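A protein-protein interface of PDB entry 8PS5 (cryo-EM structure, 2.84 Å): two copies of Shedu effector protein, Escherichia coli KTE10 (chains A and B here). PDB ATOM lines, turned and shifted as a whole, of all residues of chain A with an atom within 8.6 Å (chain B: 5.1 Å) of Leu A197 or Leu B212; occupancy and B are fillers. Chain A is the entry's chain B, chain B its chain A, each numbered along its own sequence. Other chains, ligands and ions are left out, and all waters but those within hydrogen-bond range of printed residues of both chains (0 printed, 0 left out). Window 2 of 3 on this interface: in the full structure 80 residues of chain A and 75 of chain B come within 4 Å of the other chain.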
ATOM      1  N   ILE A 191      23.179   1.461  18.895  1.00  0.00           N
ATOM      2  CA  ILE A 191      23.943   2.705  18.780  1.00  0.00           C
ATOM      3  C   ILE A 191      24.803   2.952  20.022  1.00  0.00           C
ATOM      4  O   ILE A 191      26.008   3.210  19.912  1.00  0.00           O
ATOM      5  CB  ILE A 191      22.983   3.876  18.486  1.00  0.00           C
ATOM      6  CG1 ILE A 191      22.579   3.863  17.013  1.00  0.00           C
ATOM      7  CG2 ILE A 191      23.605   5.225  18.813  1.00  0.00           C
ATOM      8  CD1 ILE A 191      21.508   4.861  16.667  1.00  0.00           C
ATOM      9  N   ARG A 192      24.221   2.841  21.217  1.00  0.00           N
ATOM     10  CA  ARG A 192      24.947   3.155  22.452  1.00  0.00           C
ATOM     11  C   ARG A 192      25.816   1.969  22.873  1.00  0.00           C
ATOM     12  O   ARG A 192      25.473   1.174  23.750  1.00  0.00           O
ATOM     13  CB  ARG A 192      23.979   3.551  23.559  1.00  0.00           C
ATOM     14  CG  ARG A 192      23.319   4.898  23.360  1.00  0.00           C
ATOM     15  CD  ARG A 192      23.141   5.622  24.684  1.00  0.00           C
ATOM     16  NE  ARG A 192      24.417   5.922  25.322  1.00  0.00           N
ATOM     17  CZ  ARG A 192      24.550   6.315  26.581  1.00  0.00           C
ATOM     18  NH1 ARG A 192      23.501   6.468  27.372  1.00  0.00           N
ATOM     19  NH2 ARG A 192      25.766   6.563  27.059  1.00  0.00           N
ATOM     20  N   THR A 194      28.838   2.610  24.074  1.00  0.00           N
ATOM     21  CA  THR A 194      29.754   3.201  25.037  1.00  0.00           C
ATOM     22  C   THR A 194      28.938   3.987  26.055  1.00  0.00           C
ATOM     23  O   THR A 194      27.982   4.677  25.688  1.00  0.00           O
ATOM     24  CB  THR A 194      30.782   4.103  24.306  1.00  0.00           C
ATOM     25  OG1 THR A 194      31.507   3.315  23.354  1.00  0.00           O
ATOM     26  CG2 THR A 194      31.792   4.730  25.264  1.00  0.00           C
ATOM     27  N   ASP A 195      29.299   3.849  27.339  1.00  0.00           N
ATOM     28  CA  ASP A 195      28.627   4.591  28.405  1.00  0.00           C
ATOM     29  C   ASP A 195      28.910   6.090  28.308  1.00  0.00           C
ATOM     30  O   ASP A 195      28.072   6.913  28.697  1.00  0.00           O
ATOM     31  CB  ASP A 195      29.061   4.039  29.766  1.00  0.00           C
ATOM     32  CG  ASP A 195      28.359   4.716  30.928  1.00  0.00           C
ATOM     33  OD1 ASP A 195      27.116   4.622  31.011  1.00  0.00           O
ATOM     34  OD2 ASP A 195      29.050   5.344  31.758  1.00  0.00           O
ATOM     35  N   LYS A 196      30.078   6.460  27.786  1.00  0.00           N
ATOM     36  CA  LYS A 196      30.377   7.864  27.528  1.00  0.00           C
ATOM     37  C   LYS A 196      29.558   8.374  26.346  1.00  0.00           C
ATOM     38  O   LYS A 196      29.556   7.778  25.265  1.00  0.00           O
ATOM     39  CB  LYS A 196      31.873   8.041  27.258  1.00  0.00           C
ATOM     40  CG  LYS A 196      32.261   9.403  26.704  1.00  0.00           C
ATOM     41  CD  LYS A 196      32.665  10.364  27.811  1.00  0.00           C
ATOM     42  CE  LYS A 196      32.967  11.753  27.261  1.00  0.00           C
ATOM     43  NZ  LYS A 196      33.416  11.723  25.839  1.00  0.00           N
ATOM     44  N   LEU A 197      28.863   9.486  26.560  1.00  0.00           N
ATOM     45  CA  LEU A 197      27.970  10.072  25.570  1.00  0.00           C
ATOM     46  C   LEU A 197      28.736  11.088  24.733  1.00  0.00           C
ATOM     47  O   LEU A 197      29.446  11.939  25.277  1.00  0.00           O
ATOM     48  CB  LEU A 197      26.770  10.730  26.250  1.00  0.00           C
ATOM     49  CG  LEU A 197      25.581  11.130  25.380  1.00  0.00           C
ATOM     50  CD1 LEU A 197      24.798   9.907  24.949  1.00  0.00           C
ATOM     51  CD2 LEU A 197      24.691  12.088  26.146  1.00  0.00           C
ATOM     52  N   ASP A 198      28.584  10.997  23.414  1.00  0.00           N
ATOM     53  CA  ASP A 198      29.311  11.830  22.470  1.00  0.00           C
ATOM     54  C   ASP A 198      28.295  12.548  21.589  1.00  0.00           C
ATOM     55  O   ASP A 198      27.120  12.177  21.544  1.00  0.00           O
ATOM     56  CB  ASP A 198      30.289  10.974  21.637  1.00  0.00           C
ATOM     57  CG  ASP A 198      31.374  11.794  20.960  1.00  0.00           C
ATOM     58  OD1 ASP A 198      32.095  12.526  21.668  1.00  0.00           O
ATOM     59  OD2 ASP A 198      31.502  11.705  19.721  1.00  0.00           O
ATOM     60  N   LEU A 199      28.754  13.595  20.896  1.00  0.00           N
ATOM     61  CA  LEU A 199      27.853  14.441  20.117  1.00  0.00           C
ATOM     62  C   LEU A 199      27.396  13.752  18.833  1.00  0.00           C
ATOM     63  O   LEU A 199      26.312  14.047  18.318  1.00  0.00           O
ATOM     64  CB  LEU A 199      28.545  15.763  19.798  1.00  0.00           C
ATOM     65  CG  LEU A 199      28.131  16.974  20.632  1.00  0.00           C
ATOM     66  CD1 LEU A 199      29.109  18.109  20.409  1.00  0.00           C
ATOM     67  CD2 LEU A 199      26.720  17.404  20.286  1.00  0.00           C
ATOM     68  N   GLU A 200      28.217  12.850  18.293  1.00  0.00           N
ATOM     69  CA  GLU A 200      27.809  12.061  17.132  1.00  0.00           C
ATOM     70  C   GLU A 200      26.767  11.017  17.522  1.00  0.00           C
ATOM     71  O   GLU A 200      25.775  10.807  16.805  1.00  0.00           O
ATOM     72  CB  GLU A 200      29.041  11.399  16.513  1.00  0.00           C
ATOM     73  CG  GLU A 200      28.764  10.419  15.390  1.00  0.00           C
ATOM     74  CD  GLU A 200      30.004  10.118  14.574  1.00  0.00           C
ATOM     75  OE1 GLU A 200      30.003   9.109  13.837  1.00  0.00           O
ATOM     76  OE2 GLU A 200      30.983  10.888  14.673  1.00  0.00           O
ATOM     77  N   VAL A 201      26.980  10.372  18.676  1.00  0.00           N
ATOM     78  CA  VAL A 201      26.030   9.412  19.234  1.00  0.00           C
ATOM     79  C   VAL A 201      24.731  10.110  19.616  1.00  0.00           C
ATOM     80  O   VAL A 201      23.642   9.547  19.459  1.00  0.00           O
ATOM     81  CB  VAL A 201      26.667   8.691  20.439  1.00  0.00           C
ATOM     82  CG1 VAL A 201      25.855   7.479  20.850  1.00  0.00           C
ATOM     83  CG2 VAL A 201      28.093   8.283  20.114  1.00  0.00           C
ATOM     84  N   LEU A 202      24.831  11.359  20.089  1.00  0.00           N
ATOM     85  CA  LEU A 202      23.649  12.160  20.397  1.00  0.00           C
ATOM     86  C   LEU A 202      22.846  12.492  19.146  1.00  0.00           C
ATOM     87  O   LEU A 202      21.612  12.488  19.182  1.00  0.00           O
ATOM     88  CB  LEU A 202      24.058  13.447  21.111  1.00  0.00           C
ATOM     89  CG  LEU A 202      23.979  13.434  22.634  1.00  0.00           C
ATOM     90  CD1 LEU A 202      24.269  14.817  23.186  1.00  0.00           C
ATOM     91  CD2 LEU A 202      22.619  12.938  23.090  1.00  0.00           C
ATOM     92  N   ASN A 203      23.532  12.752  18.029  1.00  0.00           N
ATOM     93  CA  ASN A 203      22.841  13.014  16.768  1.00  0.00           C
ATOM     94  C   ASN A 203      22.158  11.760  16.234  1.00  0.00           C
ATOM     95  O   ASN A 203      21.044  11.837  15.699  1.00  0.00           O
ATOM     96  CB  ASN A 203      23.823  13.571  15.739  1.00  0.00           C
ATOM     97  CG  ASN A 203      23.968  15.075  15.828  1.00  0.00           C
ATOM     98  OD1 ASN A 203      23.604  15.686  16.832  1.00  0.00           O
ATOM     99  ND2 ASN A 203      24.501  15.681  14.775  1.00  0.00           N
ATOM    100  N   LEU A 205      21.032   9.307  18.170  1.00  0.00           N
ATOM    101  CA  LEU A 205      19.893   9.071  19.054  1.00  0.00           C
ATOM    102  C   LEU A 205      18.759  10.058  18.788  1.00  0.00           C
ATOM    103  O   LEU A 205      17.582   9.712  18.947  1.00  0.00           O
ATOM    104  CB  LEU A 205      20.331   9.138  20.514  1.00  0.00           C
ATOM    105  CG  LEU A 205      21.176   7.959  20.997  1.00  0.00           C
ATOM    106  CD1 LEU A 205      21.753   8.249  22.369  1.00  0.00           C
ATOM    107  CD2 LEU A 205      20.373   6.680  20.994  1.00  0.00           C
ATOM    108  N   ILE B 207      17.680  13.461  29.521  1.00  0.00           N
ATOM    109  CA  ILE B 207      18.330  13.887  30.762  1.00  0.00           C
ATOM    110  C   ILE B 207      19.847  13.863  30.608  1.00  0.00           C
ATOM    111  O   ILE B 207      20.532  14.819  30.993  1.00  0.00           O
ATOM    112  CB  ILE B 207      17.846  13.007  31.937  1.00  0.00           C
ATOM    113  CG1 ILE B 207      16.509  13.510  32.469  1.00  0.00           C
ATOM    114  CG2 ILE B 207      18.845  12.941  33.093  1.00  0.00           C
ATOM    115  CD1 ILE B 207      15.733  12.467  33.229  1.00  0.00           C
ATOM    116  N   GLU B 208      20.378  12.807  29.977  1.00  0.00           N
ATOM    117  CA  GLU B 208      21.817  12.701  29.730  1.00  0.00           C
ATOM    118  C   GLU B 208      22.301  13.746  28.729  1.00  0.00           C
ATOM    119  O   GLU B 208      23.391  14.307  28.893  1.00  0.00           O
ATOM    120  CB  GLU B 208      22.157  11.297  29.232  1.00  0.00           C
ATOM    121  CG  GLU B 208      22.771  10.399  30.286  1.00  0.00           C
ATOM    122  CD  GLU B 208      22.924   8.969  29.812  1.00  0.00           C
ATOM    123  OE1 GLU B 208      22.408   8.644  28.722  1.00  0.00           O
ATOM    124  OE2 GLU B 208      23.563   8.170  30.528  1.00  0.00           O
ATOM    125  N   LYS B 209      21.479  14.048  27.716  1.00  0.00           N
ATOM    126  CA  LYS B 209      21.811  15.060  26.715  1.00  0.00           C
ATOM    127  C   LYS B 209      21.867  16.459  27.318  1.00  0.00           C
ATOM    128  O   LYS B 209      22.857  17.185  27.143  1.00  0.00           O
ATOM    129  CB  LYS B 209      20.780  15.013  25.588  1.00  0.00           C
ATOM    130  CG  LYS B 209      20.958  16.076  24.524  1.00  0.00           C
ATOM    131  CD  LYS B 209      20.073  15.791  23.326  1.00  0.00           C
ATOM    132  CE  LYS B 209      18.619  16.094  23.621  1.00  0.00           C
ATOM    133  NZ  LYS B 209      18.354  17.552  23.632  1.00  0.00           N
ATOM    134  N   TYR B 210      20.823  16.842  28.062  1.00  0.00           N
ATOM    135  CA  TYR B 210      20.782  18.177  28.649  1.00  0.00           C
ATOM    136  C   TYR B 210      21.760  18.304  29.813  1.00  0.00           C
ATOM    137  O   TYR B 210      22.288  19.392  30.062  1.00  0.00           O
ATOM    138  CB  TYR B 210      19.357  18.513  29.085  1.00  0.00           C
ATOM    139  CG  TYR B 210      18.424  18.817  27.933  1.00  0.00           C
ATOM    140  CD1 TYR B 210      18.787  19.723  26.939  1.00  0.00           C
ATOM    141  CD2 TYR B 210      17.175  18.206  27.841  1.00  0.00           C
ATOM    142  CE1 TYR B 210      17.937  20.008  25.883  1.00  0.00           C
ATOM    143  CE2 TYR B 210      16.318  18.480  26.785  1.00  0.00           C
ATOM    144  CZ  TYR B 210      16.705  19.384  25.815  1.00  0.00           C
ATOM    145  OH  TYR B 210      15.859  19.664  24.767  1.00  0.00           O
ATOM    146  N   THR B 211      22.069  17.187  30.485  1.00  0.00           N
ATOM    147  CA  THR B 211      23.077  17.182  31.539  1.00  0.00           C
ATOM    148  C   THR B 211      24.478  17.365  30.960  1.00  0.00           C
ATOM    149  O   THR B 211      25.284  18.124  31.511  1.00  0.00           O
ATOM    150  CB  THR B 211      22.958  15.874  32.332  1.00  0.00           C
ATOM    151  OG1 THR B 211      21.689  15.839  32.996  1.00  0.00           O
ATOM    152  CG2 THR B 211      24.048  15.733  33.386  1.00  0.00           C
ATOM    153  N   LEU B 212      24.760  16.716  29.819  1.00  0.00           N
ATOM    154  CA  LEU B 212      26.039  16.884  29.129  1.00  0.00           C
ATOM    155  C   LEU B 212      26.224  18.305  28.607  1.00  0.00           C
ATOM    156  O   LEU B 212      27.309  18.887  28.755  1.00  0.00           O
ATOM    157  CB  LEU B 212      26.137  15.882  27.979  1.00  0.00           C
ATOM    158  CG  LEU B 212      27.410  15.895  27.135  1.00  0.00           C
ATOM    159  CD1 LEU B 212      28.294  14.710  27.476  1.00  0.00           C
ATOM    160  CD2 LEU B 212      27.061  15.899  25.656  1.00  0.00           C
ATOM    161  N   ILE B 213      25.161  18.887  28.036  1.00  0.00           N
ATOM    162  CA  ILE B 213      25.213  20.262  27.533  1.00  0.00           C
ATOM    163  C   ILE B 213      25.376  21.258  28.681  1.00  0.00           C
ATOM    164  O   ILE B 213      26.195  22.187  28.598  1.00  0.00           O
ATOM    165  CB  ILE B 213      23.958  20.550  26.686  1.00  0.00           C
ATOM    166  CG1 ILE B 213      24.001  19.742  25.395  1.00  0.00           C
ATOM    167  CG2 ILE B 213      23.855  22.008  26.307  1.00  0.00           C
ATOM    168  CD1 ILE B 213      22.673  19.663  24.716  1.00  0.00           C
ATOM    169  N   ARG B 214      24.656  21.037  29.791  1.00  0.00           N
ATOM    170  CA  ARG B 214      24.741  21.902  30.967  1.00  0.00           C
ATOM    171  C   ARG B 214      26.111  21.827  31.632  1.00  0.00           C
ATOM    172  O   ARG B 214      26.651  22.853  32.063  1.00  0.00           O
ATOM    173  CB  ARG B 214      23.648  21.518  31.962  1.00  0.00           C
ATOM    174  CG  ARG B 214      23.325  22.581  32.984  1.00  0.00           C
ATOM    175  CD  ARG B 214      22.838  21.974  34.284  1.00  0.00           C
ATOM    176  NE  ARG B 214      23.685  20.870  34.716  1.00  0.00           N
ATOM    177  CZ  ARG B 214      23.262  19.838  35.432  1.00  0.00           C
ATOM    178  NH1 ARG B 214      22.001  19.735  35.817  1.00  0.00           N
ATOM    179  NH2 ARG B 214      24.125  18.886  35.770  1.00  0.00           N
ATOM    180  N   ASP B 215      26.707  20.631  31.682  1.00  0.00           N
ATOM    181  CA  ASP B 215      28.031  20.476  32.275  1.00  0.00           C
ATOM    182  C   ASP B 215      29.117  21.092  31.401  1.00  0.00           C
ATOM    183  O   ASP B 215      30.064  21.690  31.925  1.00  0.00           O
ATOM    184  CB  ASP B 215      28.325  18.999  32.534  1.00  0.00           C
ATOM    185  CG  ASP B 215      27.538  18.445  33.703  1.00  0.00           C
ATOM    186  OD1 ASP B 215      26.880  19.236  34.409  1.00  0.00           O
ATOM    187  OD2 ASP B 215      27.582  17.216  33.920  1.00  0.00           O
ATOM    188  N   ILE B 216      28.983  20.985  30.071  1.00  0.00           N
ATOM    189  CA  ILE B 216      29.961  21.590  29.162  1.00  0.00           C
ATOM    190  C   ILE B 216      29.876  23.118  29.209  1.00  0.00           C
ATOM    191  O   ILE B 216      30.908  23.806  29.276  1.00  0.00           O
ATOM    192  CB  ILE B 216      29.773  21.027  27.737  1.00  0.00           C
ATOM    193  CG1 ILE B 216      30.346  19.615  27.651  1.00  0.00           C
ATOM    194  CG2 ILE B 216      30.467  21.869  26.682  1.00  0.00           C
ATOM    195  CD1 ILE B 216      29.880  18.848  26.437  1.00  0.00           C
ATOM    196  N   ILE B 217      28.653  23.664  29.266  1.00  0.00           N
ATOM    197  CA  ILE B 217      28.461  25.117  29.334  1.00  0.00           C
ATOM    198  C   ILE B 217      28.929  25.668  30.683  1.00  0.00           C
ATOM    199  O   ILE B 217      29.596  26.710  30.745  1.00  0.00           O
ATOM    200  CB  ILE B 217      26.990  25.471  29.024  1.00  0.00           C
ATOM    201  CG1 ILE B 217      26.710  25.276  27.533  1.00  0.00           C
ATOM    202  CG2 ILE B 217      26.632  26.909  29.391  1.00  0.00           C
ATOM    203  CD1 ILE B 217      25.259  25.456  27.150  1.00  0.00           C
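The side-chain carboxylate (OE1) of Glu B208 lies within salt-bridge range of the guanidinium group (NH1) of Arg A192, 2.8 Å away.
The side-chain amino group (NZ) of Lys B209 lies close to the side-chain hydroxyl (OH) of Tyr B210 (3.5 Å).
The backbone carbonyl oxygen (O) of Thr A194 sits at hydrogen-bond distance from the guanidinium group (NH2) of Arg A192, at 3.2 Å.
The guanidinium group (NH2) of Arg A192 lies within hydrogen-bond range of the backbone carbonyl oxygen (O) of Asp A195 (2.9 Å).
Among the printed residues, pairs that only touch across the chains: Leu A197 with Leu B212 (3.7 Å), Leu A202 with Lys B209 (3.7 Å), Leu A197 with Glu B208 (3.8 Å) and Leu A202 with Leu B212 (3.9 Å).
Ile A191 touches none of the printed residues of chain B.
Of the printed residues of chain B, Arg A192 touches Glu B208.
Leu A197 touches just these residues of chain B: Glu B208 (3.8 Å) and Leu B212 (3.7 Å).
Printed residues of chain B within 4 Å of Leu A202: Lys B209 and Leu B212.
Leu A205 touches none of the printed residues of chain B.
Of the printed residues of chain A, Glu B208 touches Arg A192 and Leu A197.
Of the printed residues of chain A, Lys B209 touches Leu A202.
Of chain A, only Leu A197 (3.7 Å) and Leu A202 (3.9 Å) come within 4 Å of Leu B212.
The nearest residue of chain B that does not touch Leu A197 is Lys B209 (4.1 Å).
The nearest printed residue of chain B that does not touch Arg A192 is Lys B209 (7.9 Å).
Printed residues of chain B that touch a printed residue of chain A: Glu B208, Lys B209 and Leu B212.
Of the 13 printed residues of chain A, 3 touch a printed residue of chain B.
Hydrophobic or aromatic side chains of chain A within 4 Å of the printed part of chain B: Leu A197 and Leu A202.
Among the printed residues, Asp or Glu carboxylates within 4 Å of a Lys or Arg side-chain nitrogen of the other chain: Arg A192 with Glu B208.
No position is printed for both chains.
Of the 5 pairs that touch across the chains among the printed residues, none has its exchanged pair printed and touching as well.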
